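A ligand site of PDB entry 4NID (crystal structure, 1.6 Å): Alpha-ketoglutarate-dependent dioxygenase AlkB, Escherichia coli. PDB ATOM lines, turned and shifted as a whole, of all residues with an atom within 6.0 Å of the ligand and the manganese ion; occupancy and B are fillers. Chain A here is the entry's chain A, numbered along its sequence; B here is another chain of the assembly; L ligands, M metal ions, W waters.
The manganese ion is bound by OD1 of Asp 122 (2.1 Å), NE2 of His 120 (2.2 Å), O1 of the ligand (2.2 Å), NE2 of His 176 (2.2 Å), O3 of the ligand (2.4 Å) and water W3 (2.4 Å). The manganese ion has six donor atoms within binding distance.
Water W4 lies within hydrogen-bond range of N1 of 6MA 8 of chain B (2.8 Å) and the side-chain carboxylate (OD2) of Asp 122 (2.8 Å). Water W2 lies within hydrogen-bond range of an oxygen (O4) of the ligand and the side-chain hydroxyl (OG) of Ser 134. Water W1 bridges the side-chain hydroxyl of Thr 197 (2.7 Å) and the side-chain hydroxyl of Ser 134 (2.8 Å).
The guanidinium group (NH2) of Arg 193 sits close to the side-chain amide nitrogen (ND2) of Asn 195 (3.4 Å). O4' of 6MA 8 of chain B is in hydrogen-bond range of a ring nitrogen (ND1) of His 120 (3.5 Å). The side-chain amide nitrogen (ND2) of Asn 109 lies close to the side-chain sulfur (SD) of Met 50 (3.7 Å). The backbone NH (N) of Asn 195 is in hydrogen-bond range of the backbone carbonyl oxygen (O) of Asn 109, at 2.9 Å. O of Leu 107 is in hydrogen-bond range of N of Thr 197 (2.8 Å). The side-chain hydroxyl of Ser 136 lies within hydrogen-bond range of the guanidinium group of Arg 193 (2.8 Å). N of Ile 178 sits at hydrogen-bond distance from O of Leu 117 (2.9 Å). The side-chain amide oxygen (OD1) of Asn 195 sits at hydrogen-bond distance from the side-chain hydroxyl (OG1) of Thr 197 (2.9 Å).
N1 of 6MA 8 of chain B sits close to O1 of the ligand. Residues that only touch the ligand: Ile 178, Leu 107, Leu 117, Thr 197 and Ser 134. Hydrophobic or aromatic side chains that line the ligand: Leu 107, Tyr 111, Leu 117, His 120, His 176 and Ile 178. Of the 20 residues printed, 13 come within 4 Å of the ligand.
The side-chain amide nitrogen (ND2) of Asn 195 sits at hydrogen-bond distance from an oxygen (O4) of the ligand, at 3.1 Å. The side-chain hydroxyl (OH) of Tyr 111 lies within hydrogen-bond range of an oxygen (O5) of the ligand (2.7 Å). The guanidinium group of Arg 193 is in salt-bridge range of an oxygen (O5) of the ligand (2.8 Å). O2 of the ligand sits close to OD1 of Asn 109.
Of the 20 residues printed, 3 come within 4 Å of the manganese ion.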
ATOM      1  N   MET A  50      23.181  37.668  20.922  1.00  0.00           N
ATOM      2  CA  MET A  50      23.541  36.772  19.811  1.00  0.00           C
ATOM      3  C   MET A  50      23.657  37.545  18.495  1.00  0.00           C
ATOM      4  O   MET A  50      23.010  38.576  18.309  1.00  0.00           O
ATOM      5  CB  MET A  50      22.502  35.670  19.666  1.00  0.00           C
ATOM      6  CG  MET A  50      22.565  34.671  20.812  1.00  0.00           C
ATOM      7  SD  MET A  50      21.195  33.517  20.716  1.00  0.00           S
ATOM      8  CE  MET A  50      21.738  32.121  21.699  1.00  0.00           C
ATOM      9  N   LEU A 107      26.601  30.667  14.961  1.00  0.00           N
ATOM     10  CA  LEU A 107      25.928  31.478  15.964  1.00  0.00           C
ATOM     11  C   LEU A 107      27.010  32.049  16.877  1.00  0.00           C
ATOM     12  O   LEU A 107      27.848  31.299  17.395  1.00  0.00           O
ATOM     13  CB  LEU A 107      24.943  30.616  16.740  1.00  0.00           C
ATOM     14  CG  LEU A 107      24.231  31.204  17.957  1.00  0.00           C
ATOM     15  CD1 LEU A 107      23.423  32.422  17.536  1.00  0.00           C
ATOM     16  CD2 LEU A 107      23.323  30.150  18.581  1.00  0.00           C
ATOM     17  N   ASN A 109      27.743  34.029  20.350  1.00  0.00           N
ATOM     18  CA  ASN A 109      27.103  34.276  21.643  1.00  0.00           C
ATOM     19  C   ASN A 109      28.002  35.179  22.475  1.00  0.00           C
ATOM     20  O   ASN A 109      29.194  34.942  22.548  1.00  0.00           O
ATOM     21  CB  ASN A 109      26.858  32.945  22.399  1.00  0.00           C
ATOM     22  CG  ASN A 109      25.917  32.000  21.660  1.00  0.00           C
ATOM     23  OD1 ASN A 109      26.255  30.846  21.396  1.00  0.00           O
ATOM     24  ND2 ASN A 109      24.732  32.476  21.350  1.00  0.00           N
ATOM     25  N   TYR A 111      28.366  36.638  26.341  1.00  0.00           N
ATOM     26  CA  TYR A 111      27.939  36.513  27.736  1.00  0.00           C
ATOM     27  C   TYR A 111      28.516  37.629  28.575  1.00  0.00           C
ATOM     28  O   TYR A 111      29.738  37.699  28.744  1.00  0.00           O
ATOM     29  CB  TYR A 111      28.426  35.178  28.331  1.00  0.00           C
ATOM     30  CG  TYR A 111      27.846  33.943  27.700  1.00  0.00           C
ATOM     31  CD1 TYR A 111      28.331  33.460  26.480  1.00  0.00           C
ATOM     32  CD2 TYR A 111      26.838  33.227  28.345  1.00  0.00           C
ATOM     33  CE1 TYR A 111      27.810  32.297  25.915  1.00  0.00           C
ATOM     34  CE2 TYR A 111      26.313  32.080  27.781  1.00  0.00           C
ATOM     35  CZ  TYR A 111      26.790  31.643  26.569  1.00  0.00           C
ATOM     36  OH  TYR A 111      26.221  30.503  26.050  1.00  0.00           O
ATOM     37  N   LEU A 117      22.801  30.113  29.642  1.00  0.00           N
ATOM     38  CA  LEU A 117      22.025  29.453  28.598  1.00  0.00           C
ATOM     39  C   LEU A 117      21.529  28.148  29.203  1.00  0.00           C
ATOM     40  O   LEU A 117      22.310  27.220  29.443  1.00  0.00           O
ATOM     41  CB  LEU A 117      22.882  29.251  27.338  1.00  0.00           C
ATOM     42  CG  LEU A 117      22.192  28.927  26.021  1.00  0.00           C
ATOM     43  CD1 LEU A 117      21.084  29.916  25.673  1.00  0.00           C
ATOM     44  CD2 LEU A 117      23.202  28.842  24.881  1.00  0.00           C
ATOM     45  N   HIS A 120      19.523  22.723  27.033  1.00  0.00           N
ATOM     46  CA  HIS A 120      18.772  22.626  25.814  1.00  0.00           C
ATOM     47  C   HIS A 120      19.461  21.614  24.909  1.00  0.00           C
ATOM     48  O   HIS A 120      20.570  21.155  25.183  1.00  0.00           O
ATOM     49  CB  HIS A 120      18.638  23.989  25.099  1.00  0.00           C
ATOM     50  CG  HIS A 120      19.936  24.517  24.566  1.00  0.00           C
ATOM     51  ND1 HIS A 120      20.805  25.223  25.364  1.00  0.00           N
ATOM     52  CD2 HIS A 120      20.519  24.414  23.353  1.00  0.00           C
ATOM     53  CE1 HIS A 120      21.876  25.546  24.656  1.00  0.00           C
ATOM     54  NE2 HIS A 120      21.733  25.079  23.430  1.00  0.00           N
ATOM     55  N   GLN A 121      18.770  21.230  23.838  1.00  0.00           N
ATOM     56  CA  GLN A 121      19.373  20.421  22.785  1.00  0.00           C
ATOM     57  C   GLN A 121      19.461  21.252  21.525  1.00  0.00           C
ATOM     58  O   GLN A 121      18.589  22.088  21.279  1.00  0.00           O
ATOM     59  CB  GLN A 121      18.489  19.206  22.479  1.00  0.00           C
ATOM     60  CG  GLN A 121      18.165  18.262  23.645  1.00  0.00           C
ATOM     61  CD  GLN A 121      17.083  17.256  23.266  1.00  0.00           C
ATOM     62  OE1 GLN A 121      15.891  17.582  23.226  1.00  0.00           O
ATOM     63  NE2 GLN A 121      17.499  16.027  22.956  1.00  0.00           N
ATOM     64  N   ASP A 122      20.506  21.048  20.732  1.00  0.00           N
ATOM     65  CA  ASP A 122      20.554  21.580  19.375  1.00  0.00           C
ATOM     66  C   ASP A 122      19.873  20.535  18.486  1.00  0.00           C
ATOM     67  O   ASP A 122      20.462  19.541  18.091  1.00  0.00           O
ATOM     68  CB  ASP A 122      22.018  21.843  18.938  1.00  0.00           C
ATOM     69  CG  ASP A 122      22.618  23.120  19.531  1.00  0.00           C
ATOM     70  OD1 ASP A 122      22.330  23.479  20.694  1.00  0.00           O
ATOM     71  OD2 ASP A 122      23.421  23.758  18.811  1.00  0.00           O
ATOM     72  N   SER A 134      32.052  24.053  18.930  1.00  0.00           N
ATOM     73  CA  SER A 134      31.734  25.123  19.861  1.00  0.00           C
ATOM     74  C   SER A 134      33.055  25.707  20.429  1.00  0.00           C
ATOM     75  O   SER A 134      33.775  25.007  21.136  1.00  0.00           O
ATOM     76  CB  SER A 134      30.813  24.559  20.978  1.00  0.00           C
ATOM     77  OG  SER A 134      30.252  25.580  21.783  1.00  0.00           O
ATOM     78  N   SER A 136      35.174  28.579  22.677  1.00  0.00           N
ATOM     79  CA  SER A 136      35.062  29.522  23.815  1.00  0.00           C
ATOM     80  C   SER A 136      36.148  30.565  23.698  1.00  0.00           C
ATOM     81  O   SER A 136      37.299  30.214  23.406  1.00  0.00           O
ATOM     82  CB  SER A 136      35.305  28.793  25.141  1.00  0.00           C
ATOM     83  OG  SER A 136      34.281  27.840  25.375  1.00  0.00           O
ATOM     84  N   PHE A 143      30.276  24.759  31.679  1.00  0.00           N
ATOM     85  CA  PHE A 143      29.491  24.121  30.629  1.00  0.00           C
ATOM     86  C   PHE A 143      28.892  22.869  31.211  1.00  0.00           C
ATOM     87  O   PHE A 143      29.585  22.081  31.861  1.00  0.00           O
ATOM     88  CB  PHE A 143      30.450  23.732  29.504  1.00  0.00           C
ATOM     89  CG  PHE A 143      29.798  23.064  28.309  1.00  0.00           C
ATOM     90  CD1 PHE A 143      28.840  23.725  27.548  1.00  0.00           C
ATOM     91  CD2 PHE A 143      30.245  21.809  27.894  1.00  0.00           C
ATOM     92  CE1 PHE A 143      28.273  23.105  26.428  1.00  0.00           C
ATOM     93  CE2 PHE A 143      29.704  21.208  26.771  1.00  0.00           C
ATOM     94  CZ  PHE A 143      28.718  21.861  26.049  1.00  0.00           C
ATOM     95  N   LEU A 159      35.105  25.794  30.851  1.00  0.00           N
ATOM     96  CA  LEU A 159      35.600  26.054  29.505  1.00  0.00           C
ATOM     97  C   LEU A 159      36.353  27.362  29.575  1.00  0.00           C
ATOM     98  O   LEU A 159      35.787  28.385  30.002  1.00  0.00           O
ATOM     99  CB  LEU A 159      34.461  26.161  28.492  1.00  0.00           C
ATOM    100  CG  LEU A 159      33.649  24.883  28.276  1.00  0.00           C
ATOM    101  CD1 LEU A 159      32.595  25.072  27.196  1.00  0.00           C
ATOM    102  CD2 LEU A 159      34.532  23.679  27.936  1.00  0.00           C
ATOM    103  N   TRP A 167      30.667  17.941  19.557  1.00  0.00           N
ATOM    104  CA  TRP A 167      29.826  16.754  19.748  1.00  0.00           C
ATOM    105  C   TRP A 167      29.061  16.381  18.486  1.00  0.00           C
ATOM    106  O   TRP A 167      28.821  17.230  17.621  1.00  0.00           O
ATOM    107  CB  TRP A 167      28.952  16.851  21.002  1.00  0.00           C
ATOM    108  CG  TRP A 167      27.926  17.962  21.095  1.00  0.00           C
ATOM    109  CD1 TRP A 167      26.569  17.835  20.931  1.00  0.00           C
ATOM    110  CD2 TRP A 167      28.154  19.326  21.463  1.00  0.00           C
ATOM    111  NE1 TRP A 167      25.949  19.040  21.148  1.00  0.00           N
ATOM    112  CE2 TRP A 167      26.900  19.981  21.468  1.00  0.00           C
ATOM    113  CE3 TRP A 167      29.308  20.078  21.773  1.00  0.00           C
ATOM    114  CZ2 TRP A 167      26.755  21.346  21.784  1.00  0.00           C
ATOM    115  CZ3 TRP A 167      29.167  21.426  22.088  1.00  0.00           C
ATOM    116  CH2 TRP A 167      27.899  22.053  22.084  1.00  0.00           C
ATOM    117  N   HIS A 176      22.729  20.303  26.890  1.00  0.00           N
ATOM    118  CA  HIS A 176      23.877  21.026  27.347  1.00  0.00           C
ATOM    119  C   HIS A 176      23.473  22.471  27.662  1.00  0.00           C
ATOM    120  O   HIS A 176      22.383  22.912  27.296  1.00  0.00           O
ATOM    121  CB  HIS A 176      24.962  20.987  26.274  1.00  0.00           C
ATOM    122  CG  HIS A 176      24.511  21.558  24.983  1.00  0.00           C
ATOM    123  ND1 HIS A 176      23.746  20.855  24.081  1.00  0.00           N
ATOM    124  CD2 HIS A 176      24.626  22.810  24.472  1.00  0.00           C
ATOM    125  CE1 HIS A 176      23.438  21.626  23.056  1.00  0.00           C
ATOM    126  NE2 HIS A 176      23.966  22.817  23.267  1.00  0.00           N
ATOM    127  N   GLY A 177      24.383  23.203  28.302  1.00  0.00           N
ATOM    128  CA  GLY A 177      24.065  24.553  28.756  1.00  0.00           C
ATOM    129  C   GLY A 177      25.270  25.243  29.375  1.00  0.00           C
ATOM    130  O   GLY A 177      26.351  24.639  29.525  1.00  0.00           O
ATOM    131  N   ILE A 178      25.065  26.510  29.715  1.00  0.00           N
ATOM    132  CA  ILE A 178      26.081  27.339  30.342  1.00  0.00           C
ATOM    133  C   ILE A 178      25.523  27.958  31.618  1.00  0.00           C
ATOM    134  O   ILE A 178      24.447  28.566  31.603  1.00  0.00           O
ATOM    135  CB  ILE A 178      26.562  28.442  29.363  1.00  0.00           C
ATOM    136  CG1 ILE A 178      27.381  27.849  28.186  1.00  0.00           C
ATOM    137  CG2 ILE A 178      27.364  29.508  30.109  1.00  0.00           C
ATOM    138  CD1 ILE A 178      28.800  27.404  28.521  1.00  0.00           C
ATOM    139  N   ARG A 193      32.431  36.786  27.798  1.00  0.00           N
ATOM    140  CA  ARG A 193      32.788  35.552  27.126  1.00  0.00           C
ATOM    141  C   ARG A 193      32.109  35.582  25.785  1.00  0.00           C
ATOM    142  O   ARG A 193      30.955  36.019  25.661  1.00  0.00           O
ATOM    143  CB  ARG A 193      32.295  34.349  27.935  1.00  0.00           C
ATOM    144  CG  ARG A 193      32.365  33.031  27.180  1.00  0.00           C
ATOM    145  CD  ARG A 193      32.075  31.874  28.111  1.00  0.00           C
ATOM    146  NE  ARG A 193      32.315  30.594  27.454  1.00  0.00           N
ATOM    147  CZ  ARG A 193      31.404  29.892  26.793  1.00  0.00           C
ATOM    148  NH1 ARG A 193      30.130  30.294  26.720  1.00  0.00           N
ATOM    149  NH2 ARG A 193      31.775  28.766  26.213  1.00  0.00           N
ATOM    150  N   ASN A 195      31.172  32.889  22.484  1.00  0.00           N
ATOM    151  CA  ASN A 195      31.187  31.526  22.006  1.00  0.00           C
ATOM    152  C   ASN A 195      30.806  31.489  20.528  1.00  0.00           C
ATOM    153  O   ASN A 195      29.924  32.195  20.118  1.00  0.00           O
ATOM    154  CB  ASN A 195      30.230  30.687  22.836  1.00  0.00           C
ATOM    155  CG  ASN A 195      30.236  29.244  22.417  1.00  0.00           C
ATOM    156  OD1 ASN A 195      29.419  28.841  21.603  1.00  0.00           O
ATOM    157  ND2 ASN A 195      31.185  28.479  22.923  1.00  0.00           N
ATOM    158  N   THR A 197      29.390  28.925  17.683  1.00  0.00           N
ATOM    159  CA  THR A 197      28.760  27.608  17.477  1.00  0.00           C
ATOM    160  C   THR A 197      28.575  27.398  16.003  1.00  0.00           C
ATOM    161  O   THR A 197      27.773  28.094  15.358  1.00  0.00           O
ATOM    162  CB  THR A 197      27.425  27.577  18.222  1.00  0.00           C
ATOM    163  OG1 THR A 197      27.713  27.600  19.626  1.00  0.00           O
ATOM    164  CG2 THR A 197      26.664  26.297  17.905  1.00  0.00           C
ATOM    165  P   6MA B   8      14.620  25.292  25.518  1.00  0.00           P
ATOM    166  OP1 6MA B   8      15.412  24.175  25.799  1.00  0.00           O
ATOM    167  OP2 6MA B   8      14.177  25.520  24.246  1.00  0.00           O
ATOM    168  O5' 6MA B   8      15.493  26.658  25.865  1.00  0.00           O
ATOM    169  C5' 6MA B   8      16.387  26.647  26.866  1.00  0.00           C
ATOM    170  C4' 6MA B   8      17.367  27.793  26.573  1.00  0.00           C
ATOM    171  O4' 6MA B   8      18.160  27.476  25.492  1.00  0.00           O
ATOM    172  C3' 6MA B   8      16.688  29.110  26.263  1.00  0.00           C
ATOM    173  O3' 6MA B   8      17.484  30.245  26.542  1.00  0.00           O
ATOM    174  C2' 6MA B   8      16.703  29.080  24.733  1.00  0.00           C
ATOM    175  C1' 6MA B   8      17.989  28.335  24.414  1.00  0.00           C
ATOM    176  N9  6MA B   8      18.074  27.536  23.174  1.00  0.00           N
ATOM    177  C8  6MA B   8      17.234  26.552  22.848  1.00  0.00           C
ATOM    178  N7  6MA B   8      17.602  25.985  21.726  1.00  0.00           N
ATOM    179  C5  6MA B   8      18.680  26.570  21.302  1.00  0.00           C
ATOM    180  C6  6MA B   8      19.543  26.373  20.163  1.00  0.00           C
ATOM    181  N1  6MA B   8      20.613  27.120  20.073  1.00  0.00           N
ATOM    182  C2  6MA B   8      20.830  28.059  20.988  1.00  0.00           C
ATOM    183  N3  6MA B   8      20.120  28.318  22.060  1.00  0.00           N
ATOM    184  C4  6MA B   8      19.020  27.578  22.297  1.00  0.00           C
ATOM    185  N6  6MA B   8      19.220  25.414  19.286  1.00  0.00           N
ATOM    186  C1  6MA B   8      19.965  25.333  18.055  1.00  0.00           C
HETATM  187  C1  LIG L   1      24.449  27.408  21.756  1.00  0.00           C
HETATM  188  O1  LIG L   1      23.621  26.616  21.227  1.00  0.00           O
HETATM  189  O2  LIG L   1      24.616  28.576  21.332  1.00  0.00           O
HETATM  190  C2  LIG L   1      25.234  26.928  22.886  1.00  0.00           C
HETATM  191  O3  LIG L   1      24.940  25.835  23.386  1.00  0.00           O
HETATM  192  C3  LIG L   1      26.388  27.769  23.421  1.00  0.00           C
HETATM  193  C4  LIG L   1      27.271  26.960  24.374  1.00  0.00           C
HETATM  194  C5  LIG L   1      28.429  27.815  24.875  1.00  0.00           C
HETATM  195  O4  LIG L   1      29.470  27.196  25.192  1.00  0.00           O
HETATM  196  O5  LIG L   1      28.300  29.058  25.001  1.00  0.00           O
HETATM  197 MN    MN M   1      23.392  24.615  22.088  1.00  0.00          MN
HETATM  198  O   HOH W   1      27.458  25.479  21.239  1.00  0.00           O
HETATM  199  O   HOH W   2      30.519  24.844  24.371  1.00  0.00           O
HETATM  200  O   HOH W   3      25.289  24.161  20.713  1.00  0.00           O
HETATM  201  O   HOH W   4      22.980  26.562  18.605  1.00  0.00           O
